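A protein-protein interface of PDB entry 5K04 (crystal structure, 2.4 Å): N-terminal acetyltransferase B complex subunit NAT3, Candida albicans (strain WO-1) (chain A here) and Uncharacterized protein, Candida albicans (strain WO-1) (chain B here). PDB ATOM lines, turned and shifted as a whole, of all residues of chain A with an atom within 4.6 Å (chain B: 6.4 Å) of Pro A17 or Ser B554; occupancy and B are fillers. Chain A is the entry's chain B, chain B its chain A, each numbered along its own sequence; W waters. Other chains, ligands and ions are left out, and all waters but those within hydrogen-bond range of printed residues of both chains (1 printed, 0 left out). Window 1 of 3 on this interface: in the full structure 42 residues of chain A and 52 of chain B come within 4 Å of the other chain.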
ATOM      1  N   GLU A  14      23.975  23.936   2.422  1.00  0.00           N
ATOM      2  CA  GLU A  14      22.676  24.446   1.994  1.00  0.00           C
ATOM      3  C   GLU A  14      22.544  24.482   0.476  1.00  0.00           C
ATOM      4  O   GLU A  14      21.652  25.148  -0.054  1.00  0.00           O
ATOM      5  CB  GLU A  14      22.441  25.825   2.611  1.00  0.00           C
ATOM      6  CG  GLU A  14      22.214  25.737   4.124  1.00  0.00           C
ATOM      7  CD  GLU A  14      22.289  27.078   4.821  1.00  0.00           C
ATOM      8  OE1 GLU A  14      22.636  28.080   4.160  1.00  0.00           O
ATOM      9  OE2 GLU A  14      22.004  27.133   6.033  1.00  0.00           O
ATOM     10  N   LEU A  15      23.409  23.749  -0.218  1.00  0.00           N
ATOM     11  CA  LEU A  15      23.572  23.792  -1.661  1.00  0.00           C
ATOM     12  C   LEU A  15      22.883  22.643  -2.387  1.00  0.00           C
ATOM     13  O   LEU A  15      23.030  22.525  -3.606  1.00  0.00           O
ATOM     14  CB  LEU A  15      25.066  23.764  -2.008  1.00  0.00           C
ATOM     15  CG  LEU A  15      25.791  25.095  -2.215  1.00  0.00           C
ATOM     16  CD1 LEU A  15      27.201  24.829  -2.741  1.00  0.00           C
ATOM     17  CD2 LEU A  15      25.009  26.041  -3.148  1.00  0.00           C
ATOM     18  N   ASN A  16      22.202  21.751  -1.677  1.00  0.00           N
ATOM     19  CA  ASN A  16      21.635  20.592  -2.365  1.00  0.00           C
ATOM     20  C   ASN A  16      20.630  20.960  -3.460  1.00  0.00           C
ATOM     21  O   ASN A  16      20.624  20.273  -4.496  1.00  0.00           O
ATOM     22  CB  ASN A  16      21.034  19.635  -1.333  1.00  0.00           C
ATOM     23  CG  ASN A  16      22.108  18.930  -0.505  1.00  0.00           C
ATOM     24  OD1 ASN A  16      23.257  18.787  -0.943  1.00  0.00           O
ATOM     25  ND2 ASN A  16      21.736  18.483   0.690  1.00  0.00           N
ATOM     26  N   PRO A  17      19.805  22.012  -3.335  1.00  0.00           N
ATOM     27  CA  PRO A  17      18.925  22.369  -4.463  1.00  0.00           C
ATOM     28  C   PRO A  17      19.692  22.602  -5.756  1.00  0.00           C
ATOM     29  O   PRO A  17      19.204  22.285  -6.850  1.00  0.00           O
ATOM     30  CB  PRO A  17      18.240  23.655  -3.978  1.00  0.00           C
ATOM     31  CG  PRO A  17      18.265  23.556  -2.505  1.00  0.00           C
ATOM     32  CD  PRO A  17      19.555  22.874  -2.157  1.00  0.00           C
ATOM     33  N   VAL A  18      20.911  23.118  -5.642  1.00  0.00           N
ATOM     34  CA  VAL A  18      21.769  23.300  -6.801  1.00  0.00           C
ATOM     35  C   VAL A  18      22.558  22.026  -7.105  1.00  0.00           C
ATOM     36  O   VAL A  18      22.576  21.549  -8.245  1.00  0.00           O
ATOM     37  CB  VAL A  18      22.697  24.503  -6.557  1.00  0.00           C
ATOM     38  CG1 VAL A  18      23.744  24.600  -7.651  1.00  0.00           C
ATOM     39  CG2 VAL A  18      21.880  25.784  -6.494  1.00  0.00           C
ATOM     40  N   ASN A  19      23.214  21.450  -6.098  1.00  0.00           N
ATOM     41  CA  ASN A  19      24.173  20.372  -6.337  1.00  0.00           C
ATOM     42  C   ASN A  19      23.534  18.992  -6.446  1.00  0.00           C
ATOM     43  O   ASN A  19      24.262  18.009  -6.631  1.00  0.00           O
ATOM     44  CB  ASN A  19      25.238  20.381  -5.242  1.00  0.00           C
ATOM     45  CG  ASN A  19      26.333  21.426  -5.504  1.00  0.00           C
ATOM     46  OD1 ASN A  19      26.174  22.318  -6.344  1.00  0.00           O
ATOM     47  ND2 ASN A  19      27.449  21.308  -4.784  1.00  0.00           N
ATOM     48  N   LEU A  20      22.205  18.894  -6.353  1.00  0.00           N
ATOM     49  CA  LEU A  20      21.514  17.660  -6.698  1.00  0.00           C
ATOM     50  C   LEU A  20      21.140  17.609  -8.170  1.00  0.00           C
ATOM     51  O   LEU A  20      20.650  16.569  -8.631  1.00  0.00           O
ATOM     52  CB  LEU A  20      20.252  17.478  -5.845  1.00  0.00           C
ATOM     53  CG  LEU A  20      20.474  17.053  -4.392  1.00  0.00           C
ATOM     54  CD1 LEU A  20      19.166  17.080  -3.558  1.00  0.00           C
ATOM     55  CD2 LEU A  20      21.094  15.671  -4.355  1.00  0.00           C
ATOM     56  N   GLN A  53      18.749  32.632  -0.202  1.00  0.00           N
ATOM     57  CA  GLN A  53      19.093  31.300  -0.677  1.00  0.00           C
ATOM     58  C   GLN A  53      19.994  31.411  -1.893  1.00  0.00           C
ATOM     59  O   GLN A  53      19.792  32.268  -2.755  1.00  0.00           O
ATOM     60  CB  GLN A  53      17.829  30.511  -1.031  1.00  0.00           C
ATOM     61  CG  GLN A  53      18.091  29.088  -1.523  1.00  0.00           C
ATOM     62  CD  GLN A  53      16.883  28.434  -2.201  1.00  0.00           C
ATOM     63  OE1 GLN A  53      15.910  29.098  -2.554  1.00  0.00           O
ATOM     64  NE2 GLN A  53      16.958  27.121  -2.388  1.00  0.00           N
ATOM     65  N   LEU A  81      20.454  27.258  -9.848  1.00  0.00           N
ATOM     66  CA  LEU A  81      19.242  26.587  -9.388  1.00  0.00           C
ATOM     67  C   LEU A  81      18.146  26.642 -10.453  1.00  0.00           C
ATOM     68  O   LEU A  81      17.951  27.669 -11.108  1.00  0.00           O
ATOM     69  CB  LEU A  81      18.763  27.247  -8.089  1.00  0.00           C
ATOM     70  CG  LEU A  81      17.523  26.674  -7.424  1.00  0.00           C
ATOM     71  CD1 LEU A  81      17.791  25.223  -7.116  1.00  0.00           C
ATOM     72  CD2 LEU A  81      17.170  27.476  -6.156  1.00  0.00           C
ATOM     73  N   TYR B 409      15.032  15.790  -8.915  1.00  0.00           N
ATOM     74  CA  TYR B 409      15.482  15.340  -7.608  1.00  0.00           C
ATOM     75  C   TYR B 409      14.387  15.484  -6.556  1.00  0.00           C
ATOM     76  O   TYR B 409      14.296  14.651  -5.646  1.00  0.00           O
ATOM     77  CB  TYR B 409      16.757  16.092  -7.206  1.00  0.00           C
ATOM     78  CG  TYR B 409      16.578  17.547  -6.829  1.00  0.00           C
ATOM     79  CD1 TYR B 409      16.093  17.913  -5.578  1.00  0.00           C
ATOM     80  CD2 TYR B 409      16.920  18.564  -7.709  1.00  0.00           C
ATOM     81  CE1 TYR B 409      15.936  19.249  -5.220  1.00  0.00           C
ATOM     82  CE2 TYR B 409      16.749  19.920  -7.357  1.00  0.00           C
ATOM     83  CZ  TYR B 409      16.258  20.252  -6.120  1.00  0.00           C
ATOM     84  OH  TYR B 409      16.113  21.579  -5.754  1.00  0.00           O
ATOM     85  N   LYS B 410      13.544  16.516  -6.656  1.00  0.00           N
ATOM     86  CA  LYS B 410      12.500  16.675  -5.649  1.00  0.00           C
ATOM     87  C   LYS B 410      11.559  15.481  -5.661  1.00  0.00           C
ATOM     88  O   LYS B 410      11.172  14.977  -4.602  1.00  0.00           O
ATOM     89  CB  LYS B 410      11.728  17.982  -5.857  1.00  0.00           C
ATOM     90  CG  LYS B 410      12.546  19.223  -5.501  1.00  0.00           C
ATOM     91  CD  LYS B 410      11.666  20.415  -5.173  1.00  0.00           C
ATOM     92  CE  LYS B 410      10.869  20.894  -6.348  1.00  0.00           C
ATOM     93  NZ  LYS B 410      11.723  21.394  -7.431  1.00  0.00           N
ATOM     94  N   LEU B 413      13.432  12.632  -3.935  1.00  0.00           N
ATOM     95  CA  LEU B 413      13.493  12.734  -2.479  1.00  0.00           C
ATOM     96  C   LEU B 413      12.166  12.329  -1.864  1.00  0.00           C
ATOM     97  O   LEU B 413      12.131  11.600  -0.866  1.00  0.00           O
ATOM     98  CB  LEU B 413      13.861  14.157  -2.056  1.00  0.00           C
ATOM     99  CG  LEU B 413      15.241  14.655  -2.487  1.00  0.00           C
ATOM    100  CD1 LEU B 413      15.442  16.089  -2.058  1.00  0.00           C
ATOM    101  CD2 LEU B 413      16.301  13.788  -1.913  1.00  0.00           C
ATOM    102  N   LEU B 445      22.097  14.326   3.751  1.00  0.00           N
ATOM    103  CA  LEU B 445      21.028  13.525   3.135  1.00  0.00           C
ATOM    104  C   LEU B 445      20.955  12.076   3.615  1.00  0.00           C
ATOM    105  O   LEU B 445      19.990  11.372   3.291  1.00  0.00           O
ATOM    106  CB  LEU B 445      21.196  13.536   1.602  1.00  0.00           C
ATOM    107  CG  LEU B 445      21.049  14.953   1.023  1.00  0.00           C
ATOM    108  CD1 LEU B 445      21.347  14.984  -0.473  1.00  0.00           C
ATOM    109  CD2 LEU B 445      19.638  15.522   1.337  1.00  0.00           C
ATOM    110  N   TYR B 448      17.842   9.966   4.854  1.00  0.00           N
ATOM    111  CA  TYR B 448      16.927   9.318   3.918  1.00  0.00           C
ATOM    112  C   TYR B 448      17.109   7.804   3.901  1.00  0.00           C
ATOM    113  O   TYR B 448      16.203   7.091   3.465  1.00  0.00           O
ATOM    114  CB  TYR B 448      17.112   9.875   2.490  1.00  0.00           C
ATOM    115  CG  TYR B 448      16.388  11.179   2.219  1.00  0.00           C
ATOM    116  CD1 TYR B 448      15.020  11.202   1.927  1.00  0.00           C
ATOM    117  CD2 TYR B 448      17.069  12.384   2.260  1.00  0.00           C
ATOM    118  CE1 TYR B 448      14.345  12.402   1.687  1.00  0.00           C
ATOM    119  CE2 TYR B 448      16.418  13.586   2.033  1.00  0.00           C
ATOM    120  CZ  TYR B 448      15.053  13.593   1.734  1.00  0.00           C
ATOM    121  OH  TYR B 448      14.426  14.786   1.510  1.00  0.00           O
ATOM    122  N   ASP B 551      19.399  18.065   5.861  1.00  0.00           N
ATOM    123  CA  ASP B 551      18.668  18.872   4.878  1.00  0.00           C
ATOM    124  C   ASP B 551      17.219  18.396   4.828  1.00  0.00           C
ATOM    125  O   ASP B 551      16.907  17.416   4.158  1.00  0.00           O
ATOM    126  CB  ASP B 551      19.346  18.741   3.519  1.00  0.00           C
ATOM    127  CG  ASP B 551      18.619  19.477   2.403  1.00  0.00           C
ATOM    128  OD1 ASP B 551      17.615  20.166   2.646  1.00  0.00           O
ATOM    129  OD2 ASP B 551      19.090  19.346   1.263  1.00  0.00           O
ATOM    130  N   PHE B 552      16.339  19.097   5.548  1.00  0.00           N
ATOM    131  CA  PHE B 552      14.901  18.864   5.540  1.00  0.00           C
ATOM    132  C   PHE B 552      14.159  19.850   4.645  1.00  0.00           C
ATOM    133  O   PHE B 552      12.940  19.993   4.768  1.00  0.00           O
ATOM    134  CB  PHE B 552      14.341  18.951   6.969  1.00  0.00           C
ATOM    135  CG  PHE B 552      14.949  17.957   7.920  1.00  0.00           C
ATOM    136  CD1 PHE B 552      14.768  16.598   7.729  1.00  0.00           C
ATOM    137  CD2 PHE B 552      15.704  18.379   8.999  1.00  0.00           C
ATOM    138  CE1 PHE B 552      15.322  15.677   8.603  1.00  0.00           C
ATOM    139  CE2 PHE B 552      16.271  17.466   9.868  1.00  0.00           C
ATOM    140  CZ  PHE B 552      16.080  16.113   9.678  1.00  0.00           C
ATOM    141  N   LYS B 553      14.868  20.523   3.752  1.00  0.00           N
ATOM    142  CA  LYS B 553      14.335  21.640   2.985  1.00  0.00           C
ATOM    143  C   LYS B 553      14.299  21.409   1.481  1.00  0.00           C
ATOM    144  O   LYS B 553      13.360  21.865   0.825  1.00  0.00           O
ATOM    145  CB  LYS B 553      15.162  22.910   3.273  1.00  0.00           C
ATOM    146  CG  LYS B 553      14.953  23.490   4.676  1.00  0.00           C
ATOM    147  CD  LYS B 553      15.977  24.567   4.907  1.00  0.00           C
ATOM    148  CE  LYS B 553      15.762  25.277   6.228  1.00  0.00           C
ATOM    149  NZ  LYS B 553      16.860  26.270   6.471  1.00  0.00           N
ATOM    150  N   SER B 554      15.303  20.726   0.914  1.00  0.00           N
ATOM    151  CA  SER B 554      15.453  20.667  -0.540  1.00  0.00           C
ATOM    152  C   SER B 554      14.230  20.074  -1.227  1.00  0.00           C
ATOM    153  O   SER B 554      13.890  20.489  -2.338  1.00  0.00           O
ATOM    154  CB  SER B 554      16.710  19.877  -0.902  1.00  0.00           C
ATOM    155  OG  SER B 554      17.856  20.558  -0.423  1.00  0.00           O
ATOM    156  N   GLU B 555      13.539  19.124  -0.586  1.00  0.00           N
ATOM    157  CA  GLU B 555      12.350  18.550  -1.214  1.00  0.00           C
ATOM    158  C   GLU B 555      11.158  19.494  -1.179  1.00  0.00           C
ATOM    159  O   GLU B 555      10.104  19.148  -1.732  1.00  0.00           O
ATOM    160  CB  GLU B 555      12.002  17.205  -0.556  1.00  0.00           C
ATOM    161  CG  GLU B 555      11.195  17.267   0.744  1.00  0.00           C
ATOM    162  CD  GLU B 555      12.064  17.390   1.982  1.00  0.00           C
ATOM    163  OE1 GLU B 555      13.117  18.049   1.884  1.00  0.00           O
ATOM    164  OE2 GLU B 555      11.692  16.840   3.053  1.00  0.00           O
ATOM    165  N   TRP B 556      11.313  20.671  -0.560  1.00  0.00           N
ATOM    166  CA  TRP B 556      10.271  21.690  -0.447  1.00  0.00           C
ATOM    167  C   TRP B 556      10.583  22.938  -1.252  1.00  0.00           C
ATOM    168  O   TRP B 556       9.845  23.925  -1.148  1.00  0.00           O
ATOM    169  CB  TRP B 556      10.070  22.097   1.015  1.00  0.00           C
ATOM    170  CG  TRP B 556       9.507  21.028   1.905  1.00  0.00           C
ATOM    171  CD1 TRP B 556      10.199  20.244   2.796  1.00  0.00           C
ATOM    172  CD2 TRP B 556       8.135  20.629   2.006  1.00  0.00           C
ATOM    173  NE1 TRP B 556       9.344  19.390   3.443  1.00  0.00           N
ATOM    174  CE2 TRP B 556       8.067  19.605   2.988  1.00  0.00           C
ATOM    175  CE3 TRP B 556       6.957  21.038   1.370  1.00  0.00           C
ATOM    176  CZ2 TRP B 556       6.865  18.964   3.331  1.00  0.00           C
ATOM    177  CZ3 TRP B 556       5.754  20.406   1.714  1.00  0.00           C
ATOM    178  CH2 TRP B 556       5.723  19.380   2.691  1.00  0.00           C
ATOM    179  N   ASN B 557      11.664  22.923  -2.033  1.00  0.00           N
ATOM    180  CA  ASN B 557      12.119  24.113  -2.743  1.00  0.00           C
ATOM    181  C   ASN B 557      11.068  24.555  -3.746  1.00  0.00           C
ATOM    182  O   ASN B 557      10.688  23.791  -4.637  1.00  0.00           O
ATOM    183  CB  ASN B 557      13.443  23.827  -3.447  1.00  0.00           C
ATOM    184  CG  ASN B 557      14.254  25.080  -3.697  1.00  0.00           C
ATOM    185  OD1 ASN B 557      14.846  25.639  -2.779  1.00  0.00           O
ATOM    186  ND2 ASN B 557      14.292  25.520  -4.948  1.00  0.00           N
ATOM    187  N   GLY B 558      10.574  25.785  -3.578  1.00  0.00           N
ATOM    188  CA  GLY B 558       9.508  26.293  -4.413  1.00  0.00           C
ATOM    189  C   GLY B 558       8.127  25.892  -3.963  1.00  0.00           C
ATOM    190  O   GLY B 558       7.144  26.265  -4.618  1.00  0.00           O
ATOM    191  N   LEU B 559       8.022  25.134  -2.875  1.00  0.00           N
ATOM    192  CA  LEU B 559       6.748  24.782  -2.269  1.00  0.00           C
ATOM    193  C   LEU B 559       6.673  25.405  -0.890  1.00  0.00           C
ATOM    194  O   LEU B 559       7.687  25.785  -0.299  1.00  0.00           O
ATOM    195  CB  LEU B 559       6.564  23.267  -2.129  1.00  0.00           C
ATOM    196  CG  LEU B 559       6.589  22.317  -3.318  1.00  0.00           C
ATOM    197  CD1 LEU B 559       7.991  22.152  -3.875  1.00  0.00           C
ATOM    198  CD2 LEU B 559       6.077  20.990  -2.829  1.00  0.00           C
HETATM  199  O   HOH W   1      21.151  21.662   1.495  1.00  0.00           O
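The side-chain amide nitrogen (ND2) of Asn A16 sits at hydrogen-bond distance from the side-chain carboxylate (OD2) of Asp B551 (2.8 Å). O of Pro A17 lies close to OH of Tyr B409 (3.4 Å). OD1 of Asn B557 lies within hydrogen-bond range of NE2 of Gln A53 (2.6 Å).
The side-chain carboxylate (OD2) of Asp B551 sits at hydrogen-bond distance from the side-chain hydroxyl (OG) of Ser B554 (2.4 Å). The side-chain carboxylate (OD1) of Asp B551 is in hydrogen-bond range of the backbone NH (N) of Lys B553 (3.0 Å).
Leu B445 touches Asn A16. Ser B554 touches Asn A16 (OG to CB, 3.4 Å). Pro A17 touches Ser B554. Tyr B409 touches Leu A20. Leu A20 touches Leu B445 (CD2 to CD1, 3.95 Å). Asn B557 touches Leu A81.
Printed residues of chain B within 4 Å of Asn A16: Leu B445 (3.6 Å), Asp B551 (2.8 Å) and Ser B554 (3.4 Å). Of the printed residues of chain B, Pro A17 touches Tyr B409 and Ser B554. Of the printed residues of chain B, Leu A20 touches Tyr B409 and Leu B445. Of the printed residues of chain B, Gln A53 touches Asn B557 (2.6 Å). Printed residues of chain A within 4 Å of Tyr B409: Pro A17 and Leu A20. Of the printed residues of chain A, Asp B551 touches Asn A16. Ser B554 touches just these residues of chain A: Asn A16 and Pro A17.
Along chain A the printed residues that touch a printed residue of chain B span positions 16 to 81. Printed residues of chain B that touch a printed residue of chain A: Tyr B409, Leu B445, Asp B551, Ser B554 and Asn B557. Hydrophobic or aromatic side chains of chain B within 4 Å of the printed part of chain A: Tyr B409 and Leu B445. Among the printed residues, no Asp or Glu carboxylate lies within 4 Å of a Lys or Arg side-chain nitrogen of the other chain.
Water W1 bridges the side-chain carboxylate of Asp B551 (3.1 Å) and the side-chain amide nitrogen of Asn A16 (3.3 Å).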
